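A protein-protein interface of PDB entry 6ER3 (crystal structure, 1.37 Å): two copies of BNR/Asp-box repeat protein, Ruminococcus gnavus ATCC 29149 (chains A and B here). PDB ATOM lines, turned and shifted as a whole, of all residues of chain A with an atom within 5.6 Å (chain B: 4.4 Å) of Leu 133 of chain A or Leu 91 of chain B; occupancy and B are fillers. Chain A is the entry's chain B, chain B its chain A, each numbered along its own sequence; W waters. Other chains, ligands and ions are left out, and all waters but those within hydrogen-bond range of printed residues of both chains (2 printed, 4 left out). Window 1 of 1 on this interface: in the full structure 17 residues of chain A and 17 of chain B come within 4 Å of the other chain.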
ATOM      1  N   MET A  78      -2.668 -11.704  14.809  1.00  0.00           N
ATOM      2  CA  MET A  78      -3.852 -10.944  14.406  1.00  0.00           C
ATOM      3  C   MET A  78      -3.878  -9.658  15.177  1.00  0.00           C
ATOM      4  O   MET A  78      -3.314  -9.548  16.267  1.00  0.00           O
ATOM      5  CB  MET A  78      -5.132 -11.750  14.653  1.00  0.00           C
ATOM      6  CG  MET A  78      -5.530 -11.901  16.121  1.00  0.00           C
ATOM      7  SD  MET A  78      -6.700 -10.629  16.600  1.00  0.00           S
ATOM      8  CE  MET A  78      -6.911 -10.951  18.355  1.00  0.00           C
ATOM      9  N   TYR A  89      -6.605  -5.336  20.335  1.00  0.00           N
ATOM     10  CA  TYR A  89      -6.464  -6.709  20.802  1.00  0.00           C
ATOM     11  C   TYR A  89      -5.652  -7.468  19.790  1.00  0.00           C
ATOM     12  O   TYR A  89      -6.009  -7.529  18.602  1.00  0.00           O
ATOM     13  CB  TYR A  89      -7.805  -7.417  20.886  1.00  0.00           C
ATOM     14  CG  TYR A  89      -8.735  -6.873  21.927  1.00  0.00           C
ATOM     15  CD1 TYR A  89      -8.287  -6.000  22.916  1.00  0.00           C
ATOM     16  CD2 TYR A  89     -10.044  -7.277  21.974  1.00  0.00           C
ATOM     17  CE1 TYR A  89      -9.161  -5.531  23.877  1.00  0.00           C
ATOM     18  CE2 TYR A  89     -10.915  -6.833  22.947  1.00  0.00           C
ATOM     19  CZ  TYR A  89     -10.452  -5.945  23.895  1.00  0.00           C
ATOM     20  OH  TYR A  89     -11.276  -5.446  24.868  1.00  0.00           O
ATOM     21  N   THR A  90      -4.558  -8.052  20.248  1.00  0.00           N
ATOM     22  CA  THR A  90      -3.583  -8.598  19.324  1.00  0.00           C
ATOM     23  C   THR A  90      -3.059  -9.922  19.826  1.00  0.00           C
ATOM     24  O   THR A  90      -3.025 -10.204  21.031  1.00  0.00           O
ATOM     25  CB  THR A  90      -2.374  -7.680  19.145  1.00  0.00           C
ATOM     26  OG1 THR A  90      -1.621  -7.594  20.349  1.00  0.00           O
ATOM     27  CG2 THR A  90      -2.737  -6.223  18.766  1.00  0.00           C
ATOM     28  N   LEU A  91      -2.610 -10.729  18.890  1.00  0.00           N
ATOM     29  CA  LEU A  91      -1.845 -11.947  19.209  1.00  0.00           C
ATOM     30  C   LEU A  91      -0.687 -11.939  18.256  1.00  0.00           C
ATOM     31  O   LEU A  91      -0.806 -11.476  17.109  1.00  0.00           O
ATOM     32  CB  LEU A  91      -2.650 -13.213  18.932  1.00  0.00           C
ATOM     33  CG  LEU A  91      -3.604 -13.612  20.037  1.00  0.00           C
ATOM     34  CD1 LEU A  91      -4.503 -14.762  19.618  1.00  0.00           C
ATOM     35  CD2 LEU A  91      -2.861 -13.943  21.335  1.00  0.00           C
ATOM     36  N   LYS A 119     -15.563 -15.282  25.449  1.00  0.00           N
ATOM     37  CA  LYS A 119     -14.723 -14.047  25.378  1.00  0.00           C
ATOM     38  C   LYS A 119     -13.266 -14.342  25.067  1.00  0.00           C
ATOM     39  O   LYS A 119     -12.362 -13.839  25.717  1.00  0.00           O
ATOM     40  CB  LYS A 119     -14.868 -13.248  26.667  1.00  0.00           C
ATOM     41  CG  LYS A 119     -16.280 -12.827  26.983  1.00  0.00           C
ATOM     42  CD  LYS A 119     -16.289 -11.960  28.253  1.00  0.00           C
ATOM     43  CE  LYS A 119     -17.621 -11.349  28.583  1.00  0.00           C
ATOM     44  NZ  LYS A 119     -17.400 -10.214  29.521  1.00  0.00           N
ATOM     45  N   GLN A 120     -13.063 -15.191  24.084  1.00  0.00           N
ATOM     46  CA  GLN A 120     -11.786 -15.832  23.836  1.00  0.00           C
ATOM     47  C   GLN A 120     -11.453 -15.805  22.349  1.00  0.00           C
ATOM     48  O   GLN A 120     -12.330 -15.963  21.516  1.00  0.00           O
ATOM     49  CB  GLN A 120     -11.898 -17.259  24.375  1.00  0.00           C
ATOM     50  CG  GLN A 120     -10.660 -18.066  24.512  1.00  0.00           C
ATOM     51  CD  GLN A 120     -10.964 -19.283  25.427  1.00  0.00           C
ATOM     52  OE1 GLN A 120     -10.386 -19.427  26.497  1.00  0.00           O
ATOM     53  NE2 GLN A 120     -11.893 -20.125  25.006  1.00  0.00           N
ATOM     54  N   TYR A 121     -10.177 -15.643  22.044  1.00  0.00           N
ATOM     55  CA  TYR A 121      -9.608 -15.729  20.712  1.00  0.00           C
ATOM     56  C   TYR A 121      -8.551 -16.818  20.758  1.00  0.00           C
ATOM     57  O   TYR A 121      -7.762 -16.843  21.680  1.00  0.00           O
ATOM     58  CB  TYR A 121      -8.950 -14.427  20.290  1.00  0.00           C
ATOM     59  CG  TYR A 121      -9.802 -13.203  20.536  1.00  0.00           C
ATOM     60  CD1 TYR A 121      -9.732 -12.530  21.733  1.00  0.00           C
ATOM     61  CD2 TYR A 121     -10.625 -12.689  19.536  1.00  0.00           C
ATOM     62  CE1 TYR A 121     -10.520 -11.408  21.960  1.00  0.00           C
ATOM     63  CE2 TYR A 121     -11.395 -11.570  19.750  1.00  0.00           C
ATOM     64  CZ  TYR A 121     -11.311 -10.933  20.969  1.00  0.00           C
ATOM     65  OH  TYR A 121     -12.092  -9.828  21.236  1.00  0.00           O
ATOM     66  N   LYS A 122      -8.544 -17.696  19.761  1.00  0.00           N
ATOM     67  CA  LYS A 122      -7.519 -18.727  19.701  1.00  0.00           C
ATOM     68  C   LYS A 122      -6.926 -18.778  18.316  1.00  0.00           C
ATOM     69  O   LYS A 122      -7.656 -18.732  17.335  1.00  0.00           O
ATOM     70  CB  LYS A 122      -8.050 -20.118  20.078  1.00  0.00           C
ATOM     71  CG  LYS A 122      -8.477 -20.268  21.511  1.00  0.00           C
ATOM     72  CD  LYS A 122      -8.658 -21.704  21.915  1.00  0.00           C
ATOM     73  CE  LYS A 122      -9.207 -21.839  23.313  1.00  0.00           C
ATOM     74  NZ  LYS A 122      -9.099 -23.198  23.891  1.00  0.00           N
ATOM     75  N   ALA A 131      -1.740 -19.842  20.565  1.00  0.00           N
ATOM     76  CA  ALA A 131      -2.024 -18.858  21.608  1.00  0.00           C
ATOM     77  C   ALA A 131      -3.499 -18.712  21.817  1.00  0.00           C
ATOM     78  O   ALA A 131      -4.281 -18.978  20.912  1.00  0.00           O
ATOM     79  CB  ALA A 131      -1.440 -17.488  21.251  1.00  0.00           C
ATOM     80  N   THR A 132      -3.846 -18.277  23.031  1.00  0.00           N
ATOM     81  CA  THR A 132      -5.211 -17.983  23.434  1.00  0.00           C
ATOM     82  C   THR A 132      -5.207 -16.641  24.138  1.00  0.00           C
ATOM     83  O   THR A 132      -4.327 -16.374  24.958  1.00  0.00           O
ATOM     84  CB  THR A 132      -5.779 -19.041  24.399  1.00  0.00           C
ATOM     85  OG1 THR A 132      -5.669 -20.332  23.765  1.00  0.00           O
ATOM     86  CG2 THR A 132      -7.224 -18.739  24.808  1.00  0.00           C
ATOM     87  N   LEU A 133      -6.178 -15.795  23.800  1.00  0.00           N
ATOM     88  CA  LEU A 133      -6.415 -14.523  24.467  1.00  0.00           C
ATOM     89  C   LEU A 133      -7.834 -14.466  25.009  1.00  0.00           C
ATOM     90  O   LEU A 133      -8.792 -14.700  24.289  1.00  0.00           O
ATOM     91  CB  LEU A 133      -6.188 -13.382  23.458  1.00  0.00           C
ATOM     92  CG  LEU A 133      -6.506 -11.969  23.931  1.00  0.00           C
ATOM     93  CD1 LEU A 133      -5.594 -11.584  25.086  1.00  0.00           C
ATOM     94  CD2 LEU A 133      -6.392 -11.005  22.761  1.00  0.00           C
ATOM     95  N   ASP A 134      -7.967 -14.161  26.290  1.00  0.00           N
ATOM     96  CA  ASP A 134      -9.278 -13.917  26.900  1.00  0.00           C
ATOM     97  C   ASP A 134      -9.330 -12.456  27.320  1.00  0.00           C
ATOM     98  O   ASP A 134      -8.405 -11.989  27.981  1.00  0.00           O
ATOM     99  CB  ASP A 134      -9.460 -14.790  28.135  1.00  0.00           C
ATOM    100  CG  ASP A 134      -9.586 -16.278  27.807  1.00  0.00           C
ATOM    101  OD1 ASP A 134     -10.659 -16.668  27.300  1.00  0.00           O
ATOM    102  OD2 ASP A 134      -8.643 -17.066  28.072  1.00  0.00           O
ATOM    103  N   GLN A 135     -10.331 -11.707  26.869  1.00  0.00           N
ATOM    104  CA  GLN A 135     -10.459 -10.290  27.194  1.00  0.00           C
ATOM    105  C   GLN A 135     -11.775 -10.082  27.883  1.00  0.00           C
ATOM    106  O   GLN A 135     -12.801 -10.557  27.369  1.00  0.00           O
ATOM    107  CB  GLN A 135     -10.547  -9.440  25.931  1.00  0.00           C
ATOM    108  CG  GLN A 135      -9.236  -9.199  25.274  1.00  0.00           C
ATOM    109  CD  GLN A 135      -8.326  -8.213  25.961  1.00  0.00           C
ATOM    110  OE1 GLN A 135      -8.679  -7.442  26.864  1.00  0.00           O
ATOM    111  NE2 GLN A 135      -7.100  -8.230  25.504  1.00  0.00           N
ATOM    112  N   TYR B  69       2.274  -1.097  31.580  1.00  0.00           N
ATOM    113  CA  TYR B  69       1.961   0.279  31.203  1.00  0.00           C
ATOM    114  C   TYR B  69       0.499   0.599  31.385  1.00  0.00           C
ATOM    115  O   TYR B  69      -0.352  -0.283  31.458  1.00  0.00           O
ATOM    116  CB  TYR B  69       2.425   0.637  29.780  1.00  0.00           C
ATOM    117  CG  TYR B  69       1.634  -0.035  28.691  1.00  0.00           C
ATOM    118  CD1 TYR B  69       0.434   0.511  28.212  1.00  0.00           C
ATOM    119  CD2 TYR B  69       2.093  -1.194  28.087  1.00  0.00           C
ATOM    120  CE1 TYR B  69      -0.288  -0.102  27.200  1.00  0.00           C
ATOM    121  CE2 TYR B  69       1.385  -1.803  27.066  1.00  0.00           C
ATOM    122  CZ  TYR B  69       0.183  -1.258  26.641  1.00  0.00           C
ATOM    123  OH  TYR B  69      -0.558  -1.820  25.611  1.00  0.00           O
ATOM    124  N   GLY B  77      -1.860  -2.294  30.026  1.00  0.00           N
ATOM    125  CA  GLY B  77      -1.290  -3.328  29.208  1.00  0.00           C
ATOM    126  C   GLY B  77       0.120  -3.705  29.598  1.00  0.00           C
ATOM    127  O   GLY B  77       0.676  -3.218  30.584  1.00  0.00           O
ATOM    128  N   MET B  78       0.678  -4.629  28.845  1.00  0.00           N
ATOM    129  CA  MET B  78       2.086  -5.007  28.987  1.00  0.00           C
ATOM    130  C   MET B  78       2.615  -5.378  27.642  1.00  0.00           C
ATOM    131  O   MET B  78       1.885  -5.823  26.756  1.00  0.00           O
ATOM    132  CB  MET B  78       2.266  -6.142  29.989  1.00  0.00           C
ATOM    133  CG  MET B  78       1.794  -7.517  29.522  1.00  0.00           C
ATOM    134  SD  MET B  78       3.163  -8.432  28.802  1.00  0.00           S
ATOM    135  CE  MET B  78       2.339  -9.916  28.258  1.00  0.00           C
ATOM    136  N   THR B  90       1.973  -9.400  24.155  1.00  0.00           N
ATOM    137  CA  THR B  90       1.380  -8.149  24.595  1.00  0.00           C
ATOM    138  C   THR B  90      -0.012  -8.361  25.104  1.00  0.00           C
ATOM    139  O   THR B  90      -0.702  -9.289  24.695  1.00  0.00           O
ATOM    140  CB  THR B  90       1.288  -7.129  23.447  1.00  0.00           C
ATOM    141  OG1 THR B  90       0.362  -7.572  22.456  1.00  0.00           O
ATOM    142  CG2 THR B  90       2.625  -6.865  22.756  1.00  0.00           C
ATOM    143  N   LEU B  91      -0.440  -7.449  25.974  1.00  0.00           N
ATOM    144  CA  LEU B  91      -1.837  -7.333  26.417  1.00  0.00           C
ATOM    145  C   LEU B  91      -2.177  -5.853  26.374  1.00  0.00           C
ATOM    146  O   LEU B  91      -1.330  -4.994  26.602  1.00  0.00           O
ATOM    147  CB  LEU B  91      -2.043  -7.846  27.830  1.00  0.00           C
ATOM    148  CG  LEU B  91      -2.158  -9.355  27.953  1.00  0.00           C
ATOM    149  CD1 LEU B  91      -2.153  -9.817  29.402  1.00  0.00           C
ATOM    150  CD2 LEU B  91      -3.394  -9.909  27.231  1.00  0.00           C
ATOM    151  N   ASP B  92      -3.395  -5.533  26.022  1.00  0.00           N
ATOM    152  CA  ASP B  92      -3.809  -4.158  26.058  1.00  0.00           C
ATOM    153  C   ASP B  92      -5.295  -4.135  26.279  1.00  0.00           C
ATOM    154  O   ASP B  92      -6.053  -4.622  25.437  1.00  0.00           O
ATOM    155  CB  ASP B  92      -3.482  -3.387  24.819  1.00  0.00           C
ATOM    156  CG  ASP B  92      -3.675  -1.900  25.048  1.00  0.00           C
ATOM    157  OD1 ASP B  92      -4.813  -1.454  24.986  1.00  0.00           O
ATOM    158  OD2 ASP B  92      -2.712  -1.220  25.431  1.00  0.00           O
ATOM    159  N   CYS B  93      -5.691  -3.579  27.414  1.00  0.00           N
ATOM    160  CA  CYS B  93      -7.056  -3.649  27.881  1.00  0.00           C
ATOM    161  C   CYS B  93      -7.647  -2.279  28.035  1.00  0.00           C
ATOM    162  O   CYS B  93      -7.095  -1.470  28.800  1.00  0.00           O
ATOM    163  CB  CYS B  93      -7.103  -4.305  29.240  1.00  0.00           C
ATOM    164  SG  CYS B  93      -6.471  -5.972  29.193  1.00  0.00           S
ATOM    165  N   LEU B 123      -3.616 -10.212  33.665  1.00  0.00           N
ATOM    166  CA  LEU B 123      -3.622  -8.810  34.018  1.00  0.00           C
ATOM    167  C   LEU B 123      -4.841  -8.491  34.845  1.00  0.00           C
ATOM    168  O   LEU B 123      -5.966  -8.938  34.528  1.00  0.00           O
ATOM    169  CB  LEU B 123      -3.675  -8.018  32.717  1.00  0.00           C
ATOM    170  CG  LEU B 123      -3.273  -6.570  32.719  1.00  0.00           C
ATOM    171  CD1 LEU B 123      -1.842  -6.297  33.217  1.00  0.00           C
ATOM    172  CD2 LEU B 123      -3.408  -6.056  31.279  1.00  0.00           C
ATOM    173  N   ALA B 131      -7.641  -9.617  31.587  1.00  0.00           N
ATOM    174  CA  ALA B 131      -7.247 -10.378  30.424  1.00  0.00           C
ATOM    175  C   ALA B 131      -6.314 -11.491  30.820  1.00  0.00           C
ATOM    176  O   ALA B 131      -5.633 -11.434  31.823  1.00  0.00           O
ATOM    177  CB  ALA B 131      -6.563  -9.509  29.374  1.00  0.00           C
ATOM    178  N   THR B 132      -6.299 -12.537  29.996  1.00  0.00           N
ATOM    179  CA  THR B 132      -5.430 -13.675  30.169  1.00  0.00           C
ATOM    180  C   THR B 132      -4.841 -13.988  28.794  1.00  0.00           C
ATOM    181  O   THR B 132      -5.561 -13.992  27.784  1.00  0.00           O
ATOM    182  CB  THR B 132      -6.205 -14.923  30.669  1.00  0.00           C
ATOM    183  OG1 THR B 132      -6.955 -14.608  31.865  1.00  0.00           O
ATOM    184  CG2 THR B 132      -5.267 -16.121  30.898  1.00  0.00           C
ATOM    185  N   LEU B 133      -3.537 -14.251  28.752  1.00  0.00           N
ATOM    186  CA  LEU B 133      -2.833 -14.666  27.543  1.00  0.00           C
ATOM    187  C   LEU B 133      -2.122 -15.977  27.774  1.00  0.00           C
ATOM    188  O   LEU B 133      -1.371 -16.102  28.740  1.00  0.00           O
ATOM    189  CB  LEU B 133      -1.819 -13.606  27.163  1.00  0.00           C
ATOM    190  CG  LEU B 133      -0.883 -13.935  25.999  1.00  0.00           C
ATOM    191  CD1 LEU B 133      -1.694 -14.108  24.724  1.00  0.00           C
ATOM    192  CD2 LEU B 133       0.167 -12.852  25.843  1.00  0.00           C
HETATM  193  O   HOH W   1      -1.821  -6.342  23.084  1.00  0.00           O
HETATM  194  O   HOH W   2       0.126  -9.237  19.924  1.00  0.00           O
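N of Asp 134 of chain A lies within hydrogen-bond range of O of Thr 132 of chain B, 2.8 Å away.
OG1 of Thr 90 of chain A lies within hydrogen-bond range of OG1 of Thr 90 of chain B, 2.9 Å away.
The side-chain sulfur (SG) of Cys 93 of chain B lies within hydrogen-bond range of the side-chain amide oxygen (OE1) of Gln 135 of chain A (3.5 Å).
The side-chain amide oxygen of Gln 120 of chain A lies close to the side-chain carboxylate of Asp 134 of chain A, at 2.9 Å.
The backbone NH (N) of Leu 91 of chain A is in hydrogen-bond range of the backbone carbonyl oxygen (O) of Met 78 of chain A.
N of Gln 135 of chain A is in hydrogen-bond range of O of Lys 119 of chain A, at 3.2 Å.
The backbone NH (N) of Tyr 121 of chain A is in hydrogen-bond range of the backbone carbonyl oxygen (O) of Leu 133 of chain A, 2.8 Å away.
OH of Tyr 69 of chain B sits at hydrogen-bond distance from O of Leu 91 of chain B.
The backbone carbonyl oxygen (O) of Met 78 of chain B sits at hydrogen-bond distance from the backbone NH (N) of Leu 91 of chain B, 2.9 Å away.
Among the printed residues, pairs that only touch across the chains: Tyr 89 of chain A with Asp 92 of chain B, Leu 91 of chain A with Leu 133 of chain B, Thr 132 of chain A with Thr 132 of chain B, Thr 132 of chain A with Leu 133 of chain B, Leu 133 of chain A with Leu 91 of chain B, Leu 133 of chain A with Thr 132 of chain B, Asp 134 of chain A with Ala 131 of chain B, Gln 135 of chain A with Asp 92 of chain B and Gln 135 of chain A with Ala 131 of chain B.
Of the printed residues of chain B, Leu 133 of chain A touches Leu 91 and Thr 132.
Leu 91 of chain B touches one residue of chain A.
Of the printed residues of chain B, Tyr 89 of chain A touches Asp 92 (3.6 Å).
Of the printed residues of chain A, Leu 133 of chain B touches Leu 91 (3.6 Å) and Thr 132 (3.4 Å).
The nearest residue of chain A that does not touch Leu 91 of chain B is Gln 135 of chain A (4.4 Å).
The nearest printed residue of chain A that does not touch Asp 92 of chain B is Thr 90 of chain A (6.3 Å).
Hydrophobic or aromatic side chains of chain B within 4 Å of the printed part of chain A: Leu 91, Ala 131 and Leu 133.
Of the 13 printed residues of chain A, 7 touch a printed residue of chain B.
Among the printed residues, no Asp or Glu carboxylate lies within 4 Å of a Lys or Arg side-chain nitrogen of the other chain.
Thr 90 of chain A touches its own counterpart, Thr 90 of chain B.
Leu 91 of chain A touches Leu 133 of chain B, and with the chains exchanged Leu 133 of chain A touches Leu 91 of chain B.
Thr 132 of chain A touches its own counterpart, Thr 132 of chain B.
Thr 132 of chain A touches Leu 133 of chain B, and with the chains exchanged Leu 133 of chain A touches Thr 132 of chain B.
Water W2 lies within hydrogen-bond range of OG1 of Thr 90 of chain A (2.4 Å), OG1 of Thr 90 of chain B (3.0 Å) and N of Leu 91 of chain A (3.3 Å).
Water W1 lies within hydrogen-bond range of the side-chain hydroxyl of Thr 90 of chain B (2.6 Å), the side-chain hydroxyl of Thr 90 of chain A (3.0 Å), the backbone NH of Leu 91 of chain B (3.4 Å) and the backbone NH of Asp 92 of chain B (3.4 Å).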
